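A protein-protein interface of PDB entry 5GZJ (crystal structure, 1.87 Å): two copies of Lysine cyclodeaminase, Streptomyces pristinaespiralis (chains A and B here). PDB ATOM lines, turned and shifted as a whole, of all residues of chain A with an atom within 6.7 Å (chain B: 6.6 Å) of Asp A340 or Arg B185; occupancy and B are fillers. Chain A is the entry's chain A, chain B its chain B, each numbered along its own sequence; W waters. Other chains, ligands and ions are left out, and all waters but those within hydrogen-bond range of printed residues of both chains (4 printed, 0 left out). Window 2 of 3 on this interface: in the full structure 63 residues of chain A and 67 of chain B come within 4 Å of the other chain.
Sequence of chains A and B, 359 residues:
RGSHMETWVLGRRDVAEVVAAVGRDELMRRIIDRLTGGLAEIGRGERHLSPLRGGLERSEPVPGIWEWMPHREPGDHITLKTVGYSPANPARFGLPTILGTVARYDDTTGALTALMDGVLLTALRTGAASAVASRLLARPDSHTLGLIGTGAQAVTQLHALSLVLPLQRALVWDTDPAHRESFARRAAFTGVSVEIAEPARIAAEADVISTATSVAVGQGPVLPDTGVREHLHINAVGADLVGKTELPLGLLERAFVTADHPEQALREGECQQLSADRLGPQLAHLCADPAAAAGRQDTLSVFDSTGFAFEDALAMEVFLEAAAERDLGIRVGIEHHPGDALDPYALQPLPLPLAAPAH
Of the 12 printed residues of chain B, 5 touch a printed residue of chain A.
Hydrophobic or aromatic side chains of chain B within 4 Å of the printed part of chain A: Pro B96 and Phe B189.
Hydrophobic or aromatic side chains of chain A that line the printed part of chain B: Pro A338, Ala A341, Leu A342 and Tyr A345.
Along chain A the printed residues that touch a printed residue of chain B span positions 338 to 345.
Among the printed residues, 8 pairs touch across the chains.
The backbone carbonyl oxygen (O) of Leu A342 is in hydrogen-bond range of the guanidinium group (NH1) of Arg B186, 3.0 Å away.
NH2 of Arg B185 is in salt-bridge range of OD2 of Asp A340, 2.9 Å away.
Asp A340 touches just these residues of chain B: Arg B185 (2.9 Å) and Arg B186 (3.3 Å).
Of the printed residues of chain A, Pro B96 touches Pro A338 and Ala A341.
Arg B185 touches one residue of chain A.
Printed residues of chain A within 4 Å of Phe B189: Tyr A345.
Val B194 touches none of the printed residues of chain A.
The nearest residue of chain A that does not touch Arg B185 is Asp A343 (5.0 Å).
Among the printed residues, merely in contact across the chains: Asp A340 with Arg B186 (3.3 Å), Tyr A345 with Phe B189 (3.6 Å), Ala A341 with Pro B96 (3.7 Å), Asp A343 with Arg B186 (3.8 Å), Ala A341 with Gly B94 (3.8 Å) and Pro A338 with Pro B96 (3.9 Å).
The side-chain hydroxyl (OG) of Ser B182 lies within hydrogen-bond range of the guanidinium group (NH2) of Arg B186.
The side-chain carboxylate (OD1) of Asp A340 sits at hydrogen-bond distance from the backbone NH (N) of Leu A342, at 3.0 Å.
OD1 of Asp A343 sits at hydrogen-bond distance from N of Tyr A345.
No position is printed for both chains.
Water W1 bridges O of Pro A338 and O of Gly B94.
Water W4 lies within hydrogen-bond range of O of Gly B94 and O of Gly A339.
Water W3 lies within hydrogen-bond range of OD2 of Asp A343 (2.8 Å), OD2 of Asp A340 (2.9 Å) and NH1 of Arg B185 (3.0 Å).
Water W2 lies within hydrogen-bond range of O of Arg B186 (2.8 Å) and OD1 of Asp A343 (2.8 Å).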
ATOM      1  N   HIS A 337     -16.324  -7.069   5.304  1.00  0.00           N
ATOM      2  CA  HIS A 337     -15.440  -7.206   6.453  1.00  0.00           C
ATOM      3  C   HIS A 337     -14.088  -7.548   5.842  1.00  0.00           C
ATOM      4  O   HIS A 337     -13.867  -8.704   5.453  1.00  0.00           O
ATOM      5  CB  HIS A 337     -15.874  -8.324   7.386  1.00  0.00           C
ATOM      6  CG  HIS A 337     -17.214  -8.081   8.022  1.00  0.00           C
ATOM      7  ND1 HIS A 337     -17.901  -9.049   8.721  1.00  0.00           N
ATOM      8  CD2 HIS A 337     -18.014  -6.996   7.999  1.00  0.00           C
ATOM      9  CE1 HIS A 337     -19.069  -8.566   9.112  1.00  0.00           C
ATOM     10  NE2 HIS A 337     -19.147  -7.302   8.717  1.00  0.00           N
ATOM     11  N   PRO A 338     -13.206  -6.561   5.729  1.00  0.00           N
ATOM     12  CA  PRO A 338     -11.913  -6.859   5.081  1.00  0.00           C
ATOM     13  C   PRO A 338     -11.054  -7.867   5.786  1.00  0.00           C
ATOM     14  O   PRO A 338     -11.060  -7.983   7.035  1.00  0.00           O
ATOM     15  CB  PRO A 338     -11.208  -5.495   5.039  1.00  0.00           C
ATOM     16  CG  PRO A 338     -11.835  -4.714   6.093  1.00  0.00           C
ATOM     17  CD  PRO A 338     -13.272  -5.175   6.217  1.00  0.00           C
ATOM     18  N   GLY A 339     -10.207  -8.528   5.007  1.00  0.00           N
ATOM     19  CA  GLY A 339      -9.311  -9.521   5.583  1.00  0.00           C
ATOM     20  C   GLY A 339      -8.367  -8.926   6.606  1.00  0.00           C
ATOM     21  O   GLY A 339      -7.977  -9.565   7.532  1.00  0.00           O
ATOM     22  N   ASP A 340      -8.110  -7.629   6.462  1.00  0.00           N
ATOM     23  CA  ASP A 340      -7.352  -6.867   7.410  1.00  0.00           C
ATOM     24  C   ASP A 340      -8.286  -5.721   7.894  1.00  0.00           C
ATOM     25  O   ASP A 340      -8.667  -4.902   7.085  1.00  0.00           O
ATOM     26  CB  ASP A 340      -6.153  -6.289   6.677  1.00  0.00           C
ATOM     27  CG  ASP A 340      -5.283  -5.416   7.527  1.00  0.00           C
ATOM     28  OD1 ASP A 340      -5.667  -5.019   8.654  1.00  0.00           O
ATOM     29  OD2 ASP A 340      -4.191  -5.065   7.004  1.00  0.00           O
ATOM     30  N   ALA A 341      -8.629  -5.709   9.168  1.00  0.00           N
ATOM     31  CA  ALA A 341      -9.574  -4.703   9.714  1.00  0.00           C
ATOM     32  C   ALA A 341      -9.146  -3.248   9.436  1.00  0.00           C
ATOM     33  O   ALA A 341     -10.000  -2.315   9.422  1.00  0.00           O
ATOM     34  CB  ALA A 341      -9.834  -4.955  11.190  1.00  0.00           C
ATOM     35  N   LEU A 342      -7.854  -3.060   9.176  1.00  0.00           N
ATOM     36  CA  LEU A 342      -7.287  -1.730   8.969  1.00  0.00           C
ATOM     37  C   LEU A 342      -7.073  -1.403   7.538  1.00  0.00           C
ATOM     38  O   LEU A 342      -6.459  -0.390   7.209  1.00  0.00           O
ATOM     39  CB  LEU A 342      -6.010  -1.520   9.761  1.00  0.00           C
ATOM     40  CG  LEU A 342      -6.056  -1.770  11.259  1.00  0.00           C
ATOM     41  CD1 LEU A 342      -4.697  -1.338  11.838  1.00  0.00           C
ATOM     42  CD2 LEU A 342      -7.198  -1.107  12.001  1.00  0.00           C
ATOM     43  N   ASP A 343      -7.571  -2.264   6.627  1.00  0.00           N
ATOM     44  CA  ASP A 343      -7.375  -2.032   5.173  1.00  0.00           C
ATOM     45  C   ASP A 343      -8.671  -2.144   4.426  1.00  0.00           C
ATOM     46  O   ASP A 343      -9.116  -3.223   4.103  1.00  0.00           O
ATOM     47  CB  ASP A 343      -6.348  -3.041   4.639  1.00  0.00           C
ATOM     48  CG  ASP A 343      -5.964  -2.820   3.174  1.00  0.00           C
ATOM     49  OD1 ASP A 343      -6.490  -1.905   2.529  1.00  0.00           O
ATOM     50  OD2 ASP A 343      -5.142  -3.684   2.639  1.00  0.00           O
ATOM     51  N   PRO A 344      -9.311  -1.009   4.138  1.00  0.00           N
ATOM     52  CA  PRO A 344     -10.574  -1.039   3.413  1.00  0.00           C
ATOM     53  C   PRO A 344     -10.482  -1.705   2.049  1.00  0.00           C
ATOM     54  O   PRO A 344     -11.478  -2.190   1.516  1.00  0.00           O
ATOM     55  CB  PRO A 344     -10.898   0.458   3.177  1.00  0.00           C
ATOM     56  CG  PRO A 344     -10.030   1.213   4.055  1.00  0.00           C
ATOM     57  CD  PRO A 344      -8.838   0.380   4.418  1.00  0.00           C
ATOM     58  N   TYR A 345      -9.281  -1.682   1.457  1.00  0.00           N
ATOM     59  CA  TYR A 345      -9.080  -2.277   0.142  1.00  0.00           C
ATOM     60  C   TYR A 345      -8.762  -3.787   0.113  1.00  0.00           C
ATOM     61  O   TYR A 345      -8.650  -4.385  -0.995  1.00  0.00           O
ATOM     62  CB  TYR A 345      -8.007  -1.536  -0.597  1.00  0.00           C
ATOM     63  CG  TYR A 345      -8.403  -0.164  -1.079  1.00  0.00           C
ATOM     64  CD1 TYR A 345      -9.425  -0.011  -1.984  1.00  0.00           C
ATOM     65  CD2 TYR A 345      -7.620   0.983  -0.776  1.00  0.00           C
ATOM     66  CE1 TYR A 345      -9.722   1.247  -2.533  1.00  0.00           C
ATOM     67  CE2 TYR A 345      -7.929   2.218  -1.315  1.00  0.00           C
ATOM     68  CZ  TYR A 345      -9.000   2.359  -2.137  1.00  0.00           C
ATOM     69  OH  TYR A 345      -9.312   3.600  -2.684  1.00  0.00           O
ATOM     70  N   ALA A 346      -8.746  -4.428   1.262  1.00  0.00           N
ATOM     71  CA  ALA A 346      -8.483  -5.896   1.339  1.00  0.00           C
ATOM     72  C   ALA A 346      -9.762  -6.623   1.025  1.00  0.00           C
ATOM     73  O   ALA A 346     -10.473  -7.125   1.902  1.00  0.00           O
ATOM     74  CB  ALA A 346      -7.944  -6.275   2.720  1.00  0.00           C
ATOM     75  N   GLN A 348      -9.975  -9.273  -1.025  1.00  0.00           N
ATOM     76  CA  GLN A 348      -9.526 -10.509  -1.669  1.00  0.00           C
ATOM     77  C   GLN A 348     -10.330 -11.688  -1.080  1.00  0.00           C
ATOM     78  O   GLN A 348     -10.533 -11.761   0.147  1.00  0.00           O
ATOM     79  CB  GLN A 348      -7.994 -10.700  -1.488  1.00  0.00           C
ATOM     80  CG  GLN A 348      -7.590 -11.124  -0.076  1.00  0.00           C
ATOM     81  CD  GLN A 348      -7.185  -9.982   0.811  1.00  0.00           C
ATOM     82  OE1 GLN A 348      -7.612  -8.824   0.587  1.00  0.00           O
ATOM     83  NE2 GLN A 348      -6.298 -10.266   1.793  1.00  0.00           N
ATOM     84  N   GLY B  94     -11.401  -8.549  15.108  1.00  0.00           N
ATOM     85  CA  GLY B  94     -10.903  -8.517  13.744  1.00  0.00           C
ATOM     86  C   GLY B  94     -11.846  -7.897  12.722  1.00  0.00           C
ATOM     87  O   GLY B  94     -11.815  -8.225  11.517  1.00  0.00           O
ATOM     88  N   PRO B  96     -13.617  -4.131  11.184  1.00  0.00           N
ATOM     89  CA  PRO B  96     -13.314  -2.706  11.139  1.00  0.00           C
ATOM     90  C   PRO B  96     -14.098  -1.948  12.207  1.00  0.00           C
ATOM     91  O   PRO B  96     -15.214  -2.380  12.578  1.00  0.00           O
ATOM     92  CB  PRO B  96     -13.727  -2.275   9.740  1.00  0.00           C
ATOM     93  CG  PRO B  96     -14.716  -3.267   9.278  1.00  0.00           C
ATOM     94  CD  PRO B  96     -14.363  -4.576   9.987  1.00  0.00           C
ATOM     95  N   GLU B 181       3.238   0.216  12.384  1.00  0.00           N
ATOM     96  CA  GLU B 181       4.186  -0.690  11.698  1.00  0.00           C
ATOM     97  C   GLU B 181       3.645  -1.437  10.499  1.00  0.00           C
ATOM     98  O   GLU B 181       4.414  -1.829   9.608  1.00  0.00           O
ATOM     99  CB  GLU B 181       4.844  -1.631  12.709  1.00  0.00           C
ATOM    100  CG  GLU B 181       5.910  -0.838  13.492  1.00  0.00           C
ATOM    101  CD  GLU B 181       6.248  -1.458  14.832  1.00  0.00           C
ATOM    102  OE1 GLU B 181       6.133  -2.712  14.971  1.00  0.00           O
ATOM    103  OE2 GLU B 181       6.663  -0.695  15.734  1.00  0.00           O
ATOM    104  N   SER B 182       2.332  -1.614  10.404  1.00  0.00           N
ATOM    105  CA  SER B 182       1.753  -2.267   9.228  1.00  0.00           C
ATOM    106  C   SER B 182       1.312  -1.272   8.166  1.00  0.00           C
ATOM    107  O   SER B 182       0.878  -1.693   7.124  1.00  0.00           O
ATOM    108  CB  SER B 182       0.552  -3.145   9.601  1.00  0.00           C
ATOM    109  OG  SER B 182      -0.465  -2.278  10.182  1.00  0.00           O
ATOM    110  N   PHE B 183       1.440   0.059   8.409  1.00  0.00           N
ATOM    111  CA  PHE B 183       0.900   1.007   7.460  1.00  0.00           C
ATOM    112  C   PHE B 183       1.642   0.958   6.106  1.00  0.00           C
ATOM    113  O   PHE B 183       1.035   1.015   5.060  1.00  0.00           O
ATOM    114  CB  PHE B 183       0.872   2.443   7.986  1.00  0.00           C
ATOM    115  CG  PHE B 183       0.090   3.366   7.110  1.00  0.00           C
ATOM    116  CD1 PHE B 183      -1.276   3.280   7.039  1.00  0.00           C
ATOM    117  CD2 PHE B 183       0.735   4.304   6.328  1.00  0.00           C
ATOM    118  CE1 PHE B 183      -1.994   4.095   6.203  1.00  0.00           C
ATOM    119  CE2 PHE B 183       0.042   5.146   5.492  1.00  0.00           C
ATOM    120  CZ  PHE B 183      -1.328   5.027   5.407  1.00  0.00           C
ATOM    121  N   ALA B 184       2.971   0.883   6.163  1.00  0.00           N
ATOM    122  CA  ALA B 184       3.744   0.764   4.904  1.00  0.00           C
ATOM    123  C   ALA B 184       3.166  -0.301   3.997  1.00  0.00           C
ATOM    124  O   ALA B 184       2.990  -0.050   2.812  1.00  0.00           O
ATOM    125  CB  ALA B 184       5.207   0.509   5.198  1.00  0.00           C
ATOM    126  N   ARG B 185       2.909  -1.508   4.509  1.00  0.00           N
ATOM    127  CA  ARG B 185       2.378  -2.576   3.663  1.00  0.00           C
ATOM    128  C   ARG B 185       1.001  -2.236   3.092  1.00  0.00           C
ATOM    129  O   ARG B 185       0.722  -2.454   1.945  1.00  0.00           O
ATOM    130  CB  ARG B 185       2.263  -3.858   4.482  1.00  0.00           C
ATOM    131  CG  ARG B 185       1.725  -5.033   3.723  1.00  0.00           C
ATOM    132  CD  ARG B 185       1.680  -6.274   4.634  1.00  0.00           C
ATOM    133  NE  ARG B 185       0.702  -6.108   5.693  1.00  0.00           N
ATOM    134  CZ  ARG B 185      -0.624  -6.062   5.465  1.00  0.00           C
ATOM    135  NH1 ARG B 185      -1.153  -6.258   4.230  1.00  0.00           N
ATOM    136  NH2 ARG B 185      -1.441  -5.882   6.476  1.00  0.00           N
ATOM    137  N   ARG B 186       0.137  -1.634   3.903  1.00  0.00           N
ATOM    138  CA  ARG B 186      -1.187  -1.288   3.448  1.00  0.00           C
ATOM    139  C   ARG B 186      -1.195  -0.090   2.465  1.00  0.00           C
ATOM    140  O   ARG B 186      -2.160   0.066   1.715  1.00  0.00           O
ATOM    141  CB  ARG B 186      -2.092  -0.995   4.683  1.00  0.00           C
ATOM    142  CG  ARG B 186      -2.534  -2.223   5.459  1.00  0.00           C
ATOM    143  CD  ARG B 186      -3.396  -1.902   6.708  1.00  0.00           C
ATOM    144  NE  ARG B 186      -2.613  -1.340   7.825  1.00  0.00           N
ATOM    145  CZ  ARG B 186      -2.833  -0.149   8.421  1.00  0.00           C
ATOM    146  NH1 ARG B 186      -3.830   0.659   8.050  1.00  0.00           N
ATOM    147  NH2 ARG B 186      -2.012   0.258   9.398  1.00  0.00           N
ATOM    148  N   ALA B 187      -0.125   0.727   2.485  1.00  0.00           N
ATOM    149  CA  ALA B 187       0.039   1.873   1.655  1.00  0.00           C
ATOM    150  C   ALA B 187       0.792   1.643   0.352  1.00  0.00           C
ATOM    151  O   ALA B 187       0.840   2.534  -0.475  1.00  0.00           O
ATOM    152  CB  ALA B 187       0.780   2.977   2.417  1.00  0.00           C
ATOM    153  N   ALA B 188       1.371   0.456   0.211  1.00  0.00           N
ATOM    154  CA  ALA B 188       2.418   0.218  -0.781  1.00  0.00           C
ATOM    155  C   ALA B 188       1.868   0.397  -2.172  1.00  0.00           C
ATOM    156  O   ALA B 188       2.594   0.849  -3.047  1.00  0.00           O
ATOM    157  CB  ALA B 188       2.990  -1.173  -0.565  1.00  0.00           C
ATOM    158  N   PHE B 189       0.570   0.110  -2.371  1.00  0.00           N
ATOM    159  CA  PHE B 189      -0.058   0.248  -3.658  1.00  0.00           C
ATOM    160  C   PHE B 189      -0.088   1.674  -4.178  1.00  0.00           C
ATOM    161  O   PHE B 189      -0.155   1.879  -5.400  1.00  0.00           O
ATOM    162  CB  PHE B 189      -1.483  -0.325  -3.635  1.00  0.00           C
ATOM    163  CG  PHE B 189      -2.527   0.618  -3.014  1.00  0.00           C
ATOM    164  CD1 PHE B 189      -2.672   0.667  -1.645  1.00  0.00           C
ATOM    165  CD2 PHE B 189      -3.294   1.482  -3.796  1.00  0.00           C
ATOM    166  CE1 PHE B 189      -3.548   1.586  -1.051  1.00  0.00           C
ATOM    167  CE2 PHE B 189      -4.219   2.331  -3.199  1.00  0.00           C
ATOM    168  CZ  PHE B 189      -4.357   2.348  -1.839  1.00  0.00           C
ATOM    169  N   VAL B 194       6.689   5.523   2.940  1.00  0.00           N
ATOM    170  CA  VAL B 194       6.151   5.687   4.278  1.00  0.00           C
ATOM    171  C   VAL B 194       7.270   5.627   5.303  1.00  0.00           C
ATOM    172  O   VAL B 194       8.082   4.705   5.282  1.00  0.00           O
ATOM    173  CB  VAL B 194       5.120   4.581   4.614  1.00  0.00           C
ATOM    174  CG1 VAL B 194       4.736   4.636   6.087  1.00  0.00           C
ATOM    175  CG2 VAL B 194       3.876   4.742   3.758  1.00  0.00           C
HETATM  176  O   HOH W   1     -12.618  -7.255   8.977  1.00  0.00           O
HETATM  177  O   HOH W   2      -4.529  -0.994   0.787  1.00  0.00           O
HETATM  178  O   HOH W   3      -4.116  -5.740   4.151  1.00  0.00           O
HETATM  179  O   HOH W   4      -9.849  -9.654  10.398  1.00  0.00           O
